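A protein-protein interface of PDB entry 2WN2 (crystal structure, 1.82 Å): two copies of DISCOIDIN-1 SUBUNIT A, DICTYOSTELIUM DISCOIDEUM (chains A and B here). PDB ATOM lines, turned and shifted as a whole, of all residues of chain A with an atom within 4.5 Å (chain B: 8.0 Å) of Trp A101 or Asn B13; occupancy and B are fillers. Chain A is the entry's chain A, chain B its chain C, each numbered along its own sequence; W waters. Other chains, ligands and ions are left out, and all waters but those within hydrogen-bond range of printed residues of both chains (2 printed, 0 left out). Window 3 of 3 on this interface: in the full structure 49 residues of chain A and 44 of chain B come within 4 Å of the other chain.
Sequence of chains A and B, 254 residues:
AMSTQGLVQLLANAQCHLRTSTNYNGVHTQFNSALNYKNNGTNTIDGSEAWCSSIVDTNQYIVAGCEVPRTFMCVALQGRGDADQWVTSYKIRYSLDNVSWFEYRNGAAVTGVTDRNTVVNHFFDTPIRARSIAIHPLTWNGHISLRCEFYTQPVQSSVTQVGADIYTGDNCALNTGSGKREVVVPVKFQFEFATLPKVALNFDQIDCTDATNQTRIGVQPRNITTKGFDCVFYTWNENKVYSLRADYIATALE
The side-chain amide oxygen (OD1) of Asn B13 is in hydrogen-bond range of the side-chain amide nitrogen (ND2) of Asn A98, 3.0 Å away. The side-chain amide oxygen (OD1) of Asn A98 lies close to the side-chain amide nitrogen (NE2) of Gln B15 (3.3 Å). The side-chain amide oxygen (OD1) of Asn B13 sits at hydrogen-bond distance from the indole nitrogen (NE1) of Trp A101, at 2.9 Å. O of Asn B13 sits at hydrogen-bond distance from OG of Ser A132 (2.7 Å). OG of Ser A132 lies within hydrogen-bond range of NE2 of Gln B15.
The side-chain hydroxyl (OG) of Ser A95 is in hydrogen-bond range of the backbone NH (N) of Asn A98 (2.9 Å). N of Ser A95 lies within hydrogen-bond range of O of Ser A132 (2.9 Å). OG of Ser A132 lies within hydrogen-bond range of ND2 of Asn A98 (3.1 Å). ND2 of Asn B13 is in hydrogen-bond range of O of Gln B9, 2.8 Å away. The backbone carbonyl oxygen (O) of Leu B10 lies within hydrogen-bond range of the backbone NH (N) of Gln B15 (2.9 Å). The guanidinium group of Arg B70 is in hydrogen-bond range of the side-chain amide oxygen of Gln B15 (2.8 Å).
Among the printed residues, merely in contact across the chains: Gly A65 with Ala B14 (3.2 Å), Asn A98 with Val B8 (3.6 Å), Val A99 with Val B8 (3.7 Å), Gly A65 with Asn B13 (3.9 Å), Val A99 with Leu B7 (3.97 Å) and Val A63 with Ala B14 (3.98 Å).
Trp A101 touches just one residue of chain B: Asn B13 (2.9 Å). Asn B13 touches four residues of chain A. Printed residues of chain A within 4 Å of Val B8: Asn A98 (3.6 Å) and Val A99 (3.7 Å). Of the printed residues of chain B, Gly A65 touches Asn B13 (3.9 Å) and Ala B14 (3.2 Å). Ala A134 touches none of the printed residues of chain B. Phe A102 touches none of the printed residues of chain B. The nearest residue of chain B that does not touch Trp A101 is Ala B12 (5.2 Å). The nearest residue of chain A that does not touch Asn B13 is Val A63 (4.4 Å). The nearest printed residue of chain B that does not touch Val A63 is Asn B13 (4.4 Å).
Printed residues of chain A that touch a printed residue of chain B: Val A63, Gly A65, Asn A98, Val A99, Trp A101 and Ser A132. Hydrophobic or aromatic side chains of chain A within 4 Å of the printed part of chain B: Val A63, Val A99 and Trp A101. Among the printed residues, 11 pairs touch across the chains.
No position is printed for both chains. Of the 11 pairs that touch across the chains among the printed residues, none has its exchanged pair printed and touching as well.
Water W2 lies within hydrogen-bond range of the backbone carbonyl oxygen of Asn A98, the side-chain amide nitrogen of Asn B13 and the backbone NH of Gln B9. Water W1 bridges the side-chain amide oxygen of Asn A98 (2.8 Å) and the guanidinium group of Arg B70 (3.0 Å).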
ATOM      1  N   VAL A  63      17.196  -6.984   0.928  1.00  0.00           N
ATOM      2  CA  VAL A  63      17.976  -6.281   1.915  1.00  0.00           C
ATOM      3  C   VAL A  63      17.079  -5.333   2.694  1.00  0.00           C
ATOM      4  O   VAL A  63      16.303  -4.595   2.087  1.00  0.00           O
ATOM      5  CB  VAL A  63      19.098  -5.430   1.253  1.00  0.00           C
ATOM      6  CG1 VAL A  63      20.006  -4.768   2.381  1.00  0.00           C
ATOM      7  CG2 VAL A  63      19.930  -6.261   0.297  1.00  0.00           C
ATOM      8  N   GLY A  65      17.435  -2.243   5.284  1.00  0.00           N
ATOM      9  CA  GLY A  65      18.433  -1.295   5.732  1.00  0.00           C
ATOM     10  C   GLY A  65      17.892  -0.339   6.783  1.00  0.00           C
ATOM     11  O   GLY A  65      16.875   0.326   6.583  1.00  0.00           O
ATOM     12  N   ARG A  93      23.083 -12.476   5.801  1.00  0.00           N
ATOM     13  CA  ARG A  93      24.292 -11.677   5.728  1.00  0.00           C
ATOM     14  C   ARG A  93      23.927 -10.331   6.302  1.00  0.00           C
ATOM     15  O   ARG A  93      22.753  -9.952   6.295  1.00  0.00           O
ATOM     16  CB  ARG A  93      24.789 -11.530   4.290  1.00  0.00           C
ATOM     17  CG  ARG A  93      25.385 -12.872   3.733  1.00  0.00           C
ATOM     18  CD  ARG A  93      25.793 -12.812   2.280  1.00  0.00           C
ATOM     19  NE  ARG A  93      26.862 -11.896   2.007  1.00  0.00           N
ATOM     20  CZ  ARG A  93      26.739 -10.663   1.542  1.00  0.00           C
ATOM     21  NH1 ARG A  93      25.560 -10.129   1.218  1.00  0.00           N
ATOM     22  NH2 ARG A  93      27.821  -9.974   1.310  1.00  0.00           N
ATOM     23  N   TYR A  94      24.916  -9.629   6.850  1.00  0.00           N
ATOM     24  CA  TYR A  94      24.626  -8.370   7.514  1.00  0.00           C
ATOM     25  C   TYR A  94      25.847  -7.490   7.575  1.00  0.00           C
ATOM     26  O   TYR A  94      26.973  -7.945   7.341  1.00  0.00           O
ATOM     27  CB  TYR A  94      24.121  -8.642   8.926  1.00  0.00           C
ATOM     28  CG  TYR A  94      25.140  -9.391   9.775  1.00  0.00           C
ATOM     29  CD1 TYR A  94      26.169  -8.727  10.423  1.00  0.00           C
ATOM     30  CD2 TYR A  94      25.108 -10.772   9.857  1.00  0.00           C
ATOM     31  CE1 TYR A  94      27.152  -9.446  11.202  1.00  0.00           C
ATOM     32  CE2 TYR A  94      26.074 -11.476  10.604  1.00  0.00           C
ATOM     33  CZ  TYR A  94      27.068 -10.800  11.273  1.00  0.00           C
ATOM     34  OH  TYR A  94      27.997 -11.532  11.980  1.00  0.00           O
ATOM     35  N   SER A  95      25.618  -6.219   7.946  1.00  0.00           N
ATOM     36  CA  SER A  95      26.680  -5.275   8.083  1.00  0.00           C
ATOM     37  C   SER A  95      26.306  -4.269   9.131  1.00  0.00           C
ATOM     38  O   SER A  95      25.181  -3.775   9.124  1.00  0.00           O
ATOM     39  CB  SER A  95      26.890  -4.509   6.792  1.00  0.00           C
ATOM     40  OG  SER A  95      27.998  -3.617   6.891  1.00  0.00           O
ATOM     41  N   ASN A  98      28.159  -0.759   7.204  1.00  0.00           N
ATOM     42  CA  ASN A  98      27.761  -0.642   5.788  1.00  0.00           C
ATOM     43  C   ASN A  98      28.952  -0.527   4.855  1.00  0.00           C
ATOM     44  O   ASN A  98      28.820  -0.023   3.749  1.00  0.00           O
ATOM     45  CB  ASN A  98      26.798   0.510   5.574  1.00  0.00           C
ATOM     46  CG  ASN A  98      25.469   0.289   6.240  1.00  0.00           C
ATOM     47  OD1 ASN A  98      24.992   1.166   6.989  1.00  0.00           O
ATOM     48  ND2 ASN A  98      24.869  -0.892   6.009  1.00  0.00           N
ATOM     49  N   VAL A  99      30.103  -1.051   5.284  1.00  0.00           N
ATOM     50  CA  VAL A  99      31.293  -1.151   4.438  1.00  0.00           C
ATOM     51  C   VAL A  99      31.660  -2.624   4.312  1.00  0.00           C
ATOM     52  O   VAL A  99      31.745  -3.141   3.197  1.00  0.00           O
ATOM     53  CB  VAL A  99      32.483  -0.262   4.950  1.00  0.00           C
ATOM     54  CG1 VAL A  99      33.690  -0.381   3.981  1.00  0.00           C
ATOM     55  CG2 VAL A  99      32.044   1.239   5.058  1.00  0.00           C
ATOM     56  N   SER A 100      31.873  -3.286   5.436  1.00  0.00           N
ATOM     57  CA  SER A 100      32.110  -4.725   5.496  1.00  0.00           C
ATOM     58  C   SER A 100      30.845  -5.467   5.876  1.00  0.00           C
ATOM     59  O   SER A 100      30.133  -5.127   6.836  1.00  0.00           O
ATOM     60  CB  SER A 100      33.229  -5.051   6.482  1.00  0.00           C
ATOM     61  OG  SER A 100      34.405  -4.341   6.116  1.00  0.00           O
ATOM     62  N   TRP A 101      30.597  -6.531   5.097  1.00  0.00           N
ATOM     63  CA  TRP A 101      29.533  -7.482   5.326  1.00  0.00           C
ATOM     64  C   TRP A 101      30.069  -8.828   5.809  1.00  0.00           C
ATOM     65  O   TRP A 101      31.223  -9.208   5.505  1.00  0.00           O
ATOM     66  CB  TRP A 101      28.757  -7.661   4.007  1.00  0.00           C
ATOM     67  CG  TRP A 101      27.801  -6.522   3.767  1.00  0.00           C
ATOM     68  CD1 TRP A 101      28.129  -5.247   3.440  1.00  0.00           C
ATOM     69  CD2 TRP A 101      26.379  -6.572   3.848  1.00  0.00           C
ATOM     70  NE1 TRP A 101      26.999  -4.472   3.350  1.00  0.00           N
ATOM     71  CE2 TRP A 101      25.906  -5.265   3.618  1.00  0.00           C
ATOM     72  CE3 TRP A 101      25.447  -7.589   4.159  1.00  0.00           C
ATOM     73  CZ2 TRP A 101      24.552  -4.953   3.610  1.00  0.00           C
ATOM     74  CZ3 TRP A 101      24.078  -7.263   4.181  1.00  0.00           C
ATOM     75  CH2 TRP A 101      23.652  -5.944   3.930  1.00  0.00           C
ATOM     76  N   PHE A 102      29.230  -9.526   6.547  1.00  0.00           N
ATOM     77  CA  PHE A 102      29.545 -10.789   7.129  1.00  0.00           C
ATOM     78  C   PHE A 102      28.411 -11.750   6.880  1.00  0.00           C
ATOM     79  O   PHE A 102      27.267 -11.329   6.747  1.00  0.00           O
ATOM     80  CB  PHE A 102      29.724 -10.619   8.632  1.00  0.00           C
ATOM     81  CG  PHE A 102      30.755  -9.590   8.960  1.00  0.00           C
ATOM     82  CD1 PHE A 102      30.381  -8.297   9.236  1.00  0.00           C
ATOM     83  CD2 PHE A 102      32.101  -9.907   8.909  1.00  0.00           C
ATOM     84  CE1 PHE A 102      31.333  -7.330   9.501  1.00  0.00           C
ATOM     85  CE2 PHE A 102      33.072  -8.939   9.175  1.00  0.00           C
ATOM     86  CZ  PHE A 102      32.682  -7.650   9.463  1.00  0.00           C
ATOM     87  N   SER A 132      22.275  -3.154   8.395  1.00  0.00           N
ATOM     88  CA  SER A 132      21.589  -3.761   7.225  1.00  0.00           C
ATOM     89  C   SER A 132      21.730  -5.249   7.283  1.00  0.00           C
ATOM     90  O   SER A 132      22.744  -5.764   7.781  1.00  0.00           O
ATOM     91  CB  SER A 132      22.164  -3.247   5.914  1.00  0.00           C
ATOM     92  OG  SER A 132      21.958  -1.864   5.784  1.00  0.00           O
ATOM     93  N   ILE A 133      20.701  -5.941   6.787  1.00  0.00           N
ATOM     94  CA  ILE A 133      20.617  -7.376   6.871  1.00  0.00           C
ATOM     95  C   ILE A 133      19.942  -7.897   5.607  1.00  0.00           C
ATOM     96  O   ILE A 133      19.127  -7.202   5.021  1.00  0.00           O
ATOM     97  CB  ILE A 133      19.877  -7.822   8.172  1.00  0.00           C
ATOM     98  CG1 ILE A 133      19.998  -9.328   8.390  1.00  0.00           C
ATOM     99  CG2 ILE A 133      18.417  -7.357   8.155  1.00  0.00           C
ATOM    100  CD1 ILE A 133      19.633  -9.794   9.910  1.00  0.00           C
ATOM    101  N   ALA A 134      20.357  -9.067   5.138  1.00  0.00           N
ATOM    102  CA  ALA A 134      19.848  -9.600   3.868  1.00  0.00           C
ATOM    103  C   ALA A 134      19.532 -11.068   3.969  1.00  0.00           C
ATOM    104  O   ALA A 134      20.264 -11.846   4.608  1.00  0.00           O
ATOM    105  CB  ALA A 134      20.861  -9.374   2.741  1.00  0.00           C
ATOM    106  N   LEU B   7      34.201   3.767   1.734  1.00  0.00           N
ATOM    107  CA  LEU B   7      32.982   4.552   1.806  1.00  0.00           C
ATOM    108  C   LEU B   7      31.759   3.637   1.784  1.00  0.00           C
ATOM    109  O   LEU B   7      31.795   2.497   1.298  1.00  0.00           O
ATOM    110  CB  LEU B   7      32.949   5.549   0.668  1.00  0.00           C
ATOM    111  CG  LEU B   7      34.131   6.521   0.592  1.00  0.00           C
ATOM    112  CD1 LEU B   7      33.912   7.403  -0.547  1.00  0.00           C
ATOM    113  CD2 LEU B   7      34.320   7.370   1.891  1.00  0.00           C
ATOM    114  N   VAL B   8      30.663   4.154   2.295  1.00  0.00           N
ATOM    115  CA  VAL B   8      29.405   3.445   2.280  1.00  0.00           C
ATOM    116  C   VAL B   8      28.730   3.688   0.949  1.00  0.00           C
ATOM    117  O   VAL B   8      28.540   4.833   0.544  1.00  0.00           O
ATOM    118  CB  VAL B   8      28.515   3.924   3.430  1.00  0.00           C
ATOM    119  CG1 VAL B   8      27.066   3.334   3.411  1.00  0.00           C
ATOM    120  CG2 VAL B   8      29.219   3.583   4.753  1.00  0.00           C
ATOM    121  N   GLN B   9      28.331   2.589   0.314  1.00  0.00           N
ATOM    122  CA  GLN B   9      27.467   2.605  -0.868  1.00  0.00           C
ATOM    123  C   GLN B   9      26.014   2.685  -0.392  1.00  0.00           C
ATOM    124  O   GLN B   9      25.439   1.703   0.069  1.00  0.00           O
ATOM    125  CB  GLN B   9      27.747   1.321  -1.669  1.00  0.00           C
ATOM    126  CG  GLN B   9      29.166   1.284  -2.162  1.00  0.00           C
ATOM    127  CD  GLN B   9      29.508   0.046  -2.941  1.00  0.00           C
ATOM    128  OE1 GLN B   9      28.635  -0.606  -3.532  1.00  0.00           O
ATOM    129  NE2 GLN B   9      30.800  -0.330  -2.903  1.00  0.00           N
ATOM    130  N   LEU B  10      25.442   3.869  -0.438  1.00  0.00           N
ATOM    131  CA  LEU B  10      24.151   4.085   0.239  1.00  0.00           C
ATOM    132  C   LEU B  10      22.985   3.241  -0.255  1.00  0.00           C
ATOM    133  O   LEU B  10      22.281   2.587   0.550  1.00  0.00           O
ATOM    134  CB  LEU B  10      23.762   5.548   0.121  1.00  0.00           C
ATOM    135  CG  LEU B  10      23.131   6.306   1.257  1.00  0.00           C
ATOM    136  CD1 LEU B  10      24.017   6.266   2.550  1.00  0.00           C
ATOM    137  CD2 LEU B  10      22.807   7.795   0.748  1.00  0.00           C
ATOM    138  N   LEU B  11      22.711   3.302  -1.568  1.00  0.00           N
ATOM    139  CA  LEU B  11      21.618   2.502  -2.141  1.00  0.00           C
ATOM    140  C   LEU B  11      21.859   0.999  -2.004  1.00  0.00           C
ATOM    141  O   LEU B  11      20.928   0.241  -1.709  1.00  0.00           O
ATOM    142  CB  LEU B  11      21.361   2.866  -3.624  1.00  0.00           C
ATOM    143  CG  LEU B  11      20.556   4.134  -3.940  1.00  0.00           C
ATOM    144  CD1 LEU B  11      21.283   5.401  -3.531  1.00  0.00           C
ATOM    145  CD2 LEU B  11      20.236   4.221  -5.452  1.00  0.00           C
ATOM    146  N   ALA B  12      23.081   0.545  -2.205  1.00  0.00           N
ATOM    147  CA  ALA B  12      23.383  -0.886  -2.132  1.00  0.00           C
ATOM    148  C   ALA B  12      23.115  -1.418  -0.737  1.00  0.00           C
ATOM    149  O   ALA B  12      22.667  -2.551  -0.578  1.00  0.00           O
ATOM    150  CB  ALA B  12      24.815  -1.189  -2.559  1.00  0.00           C
ATOM    151  N   ASN B  13      23.368  -0.565   0.267  1.00  0.00           N
ATOM    152  CA  ASN B  13      23.106  -0.912   1.667  1.00  0.00           C
ATOM    153  C   ASN B  13      21.694  -0.586   2.156  1.00  0.00           C
ATOM    154  O   ASN B  13      21.418  -0.744   3.356  1.00  0.00           O
ATOM    155  CB  ASN B  13      24.153  -0.233   2.589  1.00  0.00           C
ATOM    156  CG  ASN B  13      25.507  -0.925   2.521  1.00  0.00           C
ATOM    157  OD1 ASN B  13      25.772  -1.862   3.276  1.00  0.00           O
ATOM    158  ND2 ASN B  13      26.358  -0.471   1.611  1.00  0.00           N
ATOM    159  N   ALA B  14      20.823  -0.122   1.250  1.00  0.00           N
ATOM    160  CA  ALA B  14      19.433   0.227   1.559  1.00  0.00           C
ATOM    161  C   ALA B  14      19.360   1.248   2.705  1.00  0.00           C
ATOM    162  O   ALA B  14      18.522   1.130   3.601  1.00  0.00           O
ATOM    163  CB  ALA B  14      18.641  -1.057   1.947  1.00  0.00           C
ATOM    164  N   GLN B  15      20.289   2.199   2.686  1.00  0.00           N
ATOM    165  CA  GLN B  15      20.390   3.216   3.755  1.00  0.00           C
ATOM    166  C   GLN B  15      19.533   4.440   3.498  1.00  0.00           C
ATOM    167  O   GLN B  15      19.439   5.316   4.355  1.00  0.00           O
ATOM    168  CB  GLN B  15      21.827   3.609   3.959  1.00  0.00           C
ATOM    169  CG  GLN B  15      22.606   2.540   4.648  1.00  0.00           C
ATOM    170  CD  GLN B  15      22.210   2.455   6.076  1.00  0.00           C
ATOM    171  OE1 GLN B  15      22.380   3.444   6.847  1.00  0.00           O
ATOM    172  NE2 GLN B  15      21.688   1.303   6.461  1.00  0.00           N
ATOM    173  N   CYS B  16      18.870   4.514   2.354  1.00  0.00           N
ATOM    174  CA  CYS B  16      18.030   5.695   2.062  1.00  0.00           C
ATOM    175  C   CYS B  16      16.641   5.295   1.546  1.00  0.00           C
ATOM    176  O   CYS B  16      16.454   4.243   0.948  1.00  0.00           O
ATOM    177  CB  CYS B  16      18.723   6.646   1.055  1.00  0.00           C
ATOM    178  SG  CYS B  16      19.217   5.814  -0.399  1.00  0.00           S
ATOM    179  N   ALA B  34      19.666   1.026  -8.482  1.00  0.00           N
ATOM    180  CA  ALA B  34      21.008   0.767  -7.937  1.00  0.00           C
ATOM    181  C   ALA B  34      22.066   0.605  -9.036  1.00  0.00           C
ATOM    182  O   ALA B  34      21.840  -0.078 -10.030  1.00  0.00           O
ATOM    183  CB  ALA B  34      21.014  -0.432  -7.055  1.00  0.00           C
ATOM    184  N   ARG B  70      24.808  12.656   6.671  1.00  0.00           N
ATOM    185  CA  ARG B  70      25.916  11.954   6.070  1.00  0.00           C
ATOM    186  C   ARG B  70      26.861  12.978   5.445  1.00  0.00           C
ATOM    187  O   ARG B  70      26.448  14.079   5.143  1.00  0.00           O
ATOM    188  CB  ARG B  70      25.447  11.045   4.943  1.00  0.00           C
ATOM    189  CG  ARG B  70      24.351  10.023   5.286  1.00  0.00           C
ATOM    190  CD  ARG B  70      24.786   9.048   6.298  1.00  0.00           C
ATOM    191  NE  ARG B  70      23.642   8.211   6.701  1.00  0.00           N
ATOM    192  CZ  ARG B  70      23.615   6.876   6.685  1.00  0.00           C
ATOM    193  NH1 ARG B  70      24.653   6.175   6.282  1.00  0.00           N
ATOM    194  NH2 ARG B  70      22.531   6.251   7.122  1.00  0.00           N
ATOM    195  N   GLU B 149      24.661   5.690  -7.565  1.00  0.00           N
ATOM    196  CA  GLU B 149      25.022   5.424  -6.189  1.00  0.00           C
ATOM    197  C   GLU B 149      25.536   6.725  -5.564  1.00  0.00           C
ATOM    198  O   GLU B 149      26.095   7.608  -6.260  1.00  0.00           O
ATOM    199  CB  GLU B 149      26.070   4.304  -6.099  1.00  0.00           C
ATOM    200  CG  GLU B 149      26.459   3.910  -4.709  1.00  0.00           C
ATOM    201  CD  GLU B 149      25.302   3.380  -3.898  1.00  0.00           C
ATOM    202  OE1 GLU B 149      25.141   2.143  -3.728  1.00  0.00           O
ATOM    203  OE2 GLU B 149      24.535   4.233  -3.430  1.00  0.00           O
ATOM    204  N   PHE B 150      25.337   6.835  -4.244  1.00  0.00           N
ATOM    205  CA  PHE B 150      25.987   7.875  -3.436  1.00  0.00           C
ATOM    206  C   PHE B 150      26.950   7.212  -2.455  1.00  0.00           C
ATOM    207  O   PHE B 150      26.658   6.146  -1.886  1.00  0.00           O
ATOM    208  CB  PHE B 150      24.970   8.713  -2.676  1.00  0.00           C
ATOM    209  CG  PHE B 150      24.048   9.478  -3.538  1.00  0.00           C
ATOM    210  CD1 PHE B 150      22.785   8.967  -3.836  1.00  0.00           C
ATOM    211  CD2 PHE B 150      24.407  10.717  -4.051  1.00  0.00           C
ATOM    212  CE1 PHE B 150      21.910   9.680  -4.652  1.00  0.00           C
ATOM    213  CE2 PHE B 150      23.529  11.448  -4.875  1.00  0.00           C
ATOM    214  CZ  PHE B 150      22.294  10.910  -5.201  1.00  0.00           C
HETATM  215  O   HOH W   1      26.068   3.723   7.131  1.00  0.00           O
HETATM  216  O   HOH W   2      29.239  -0.207   1.082  1.00  0.00           O
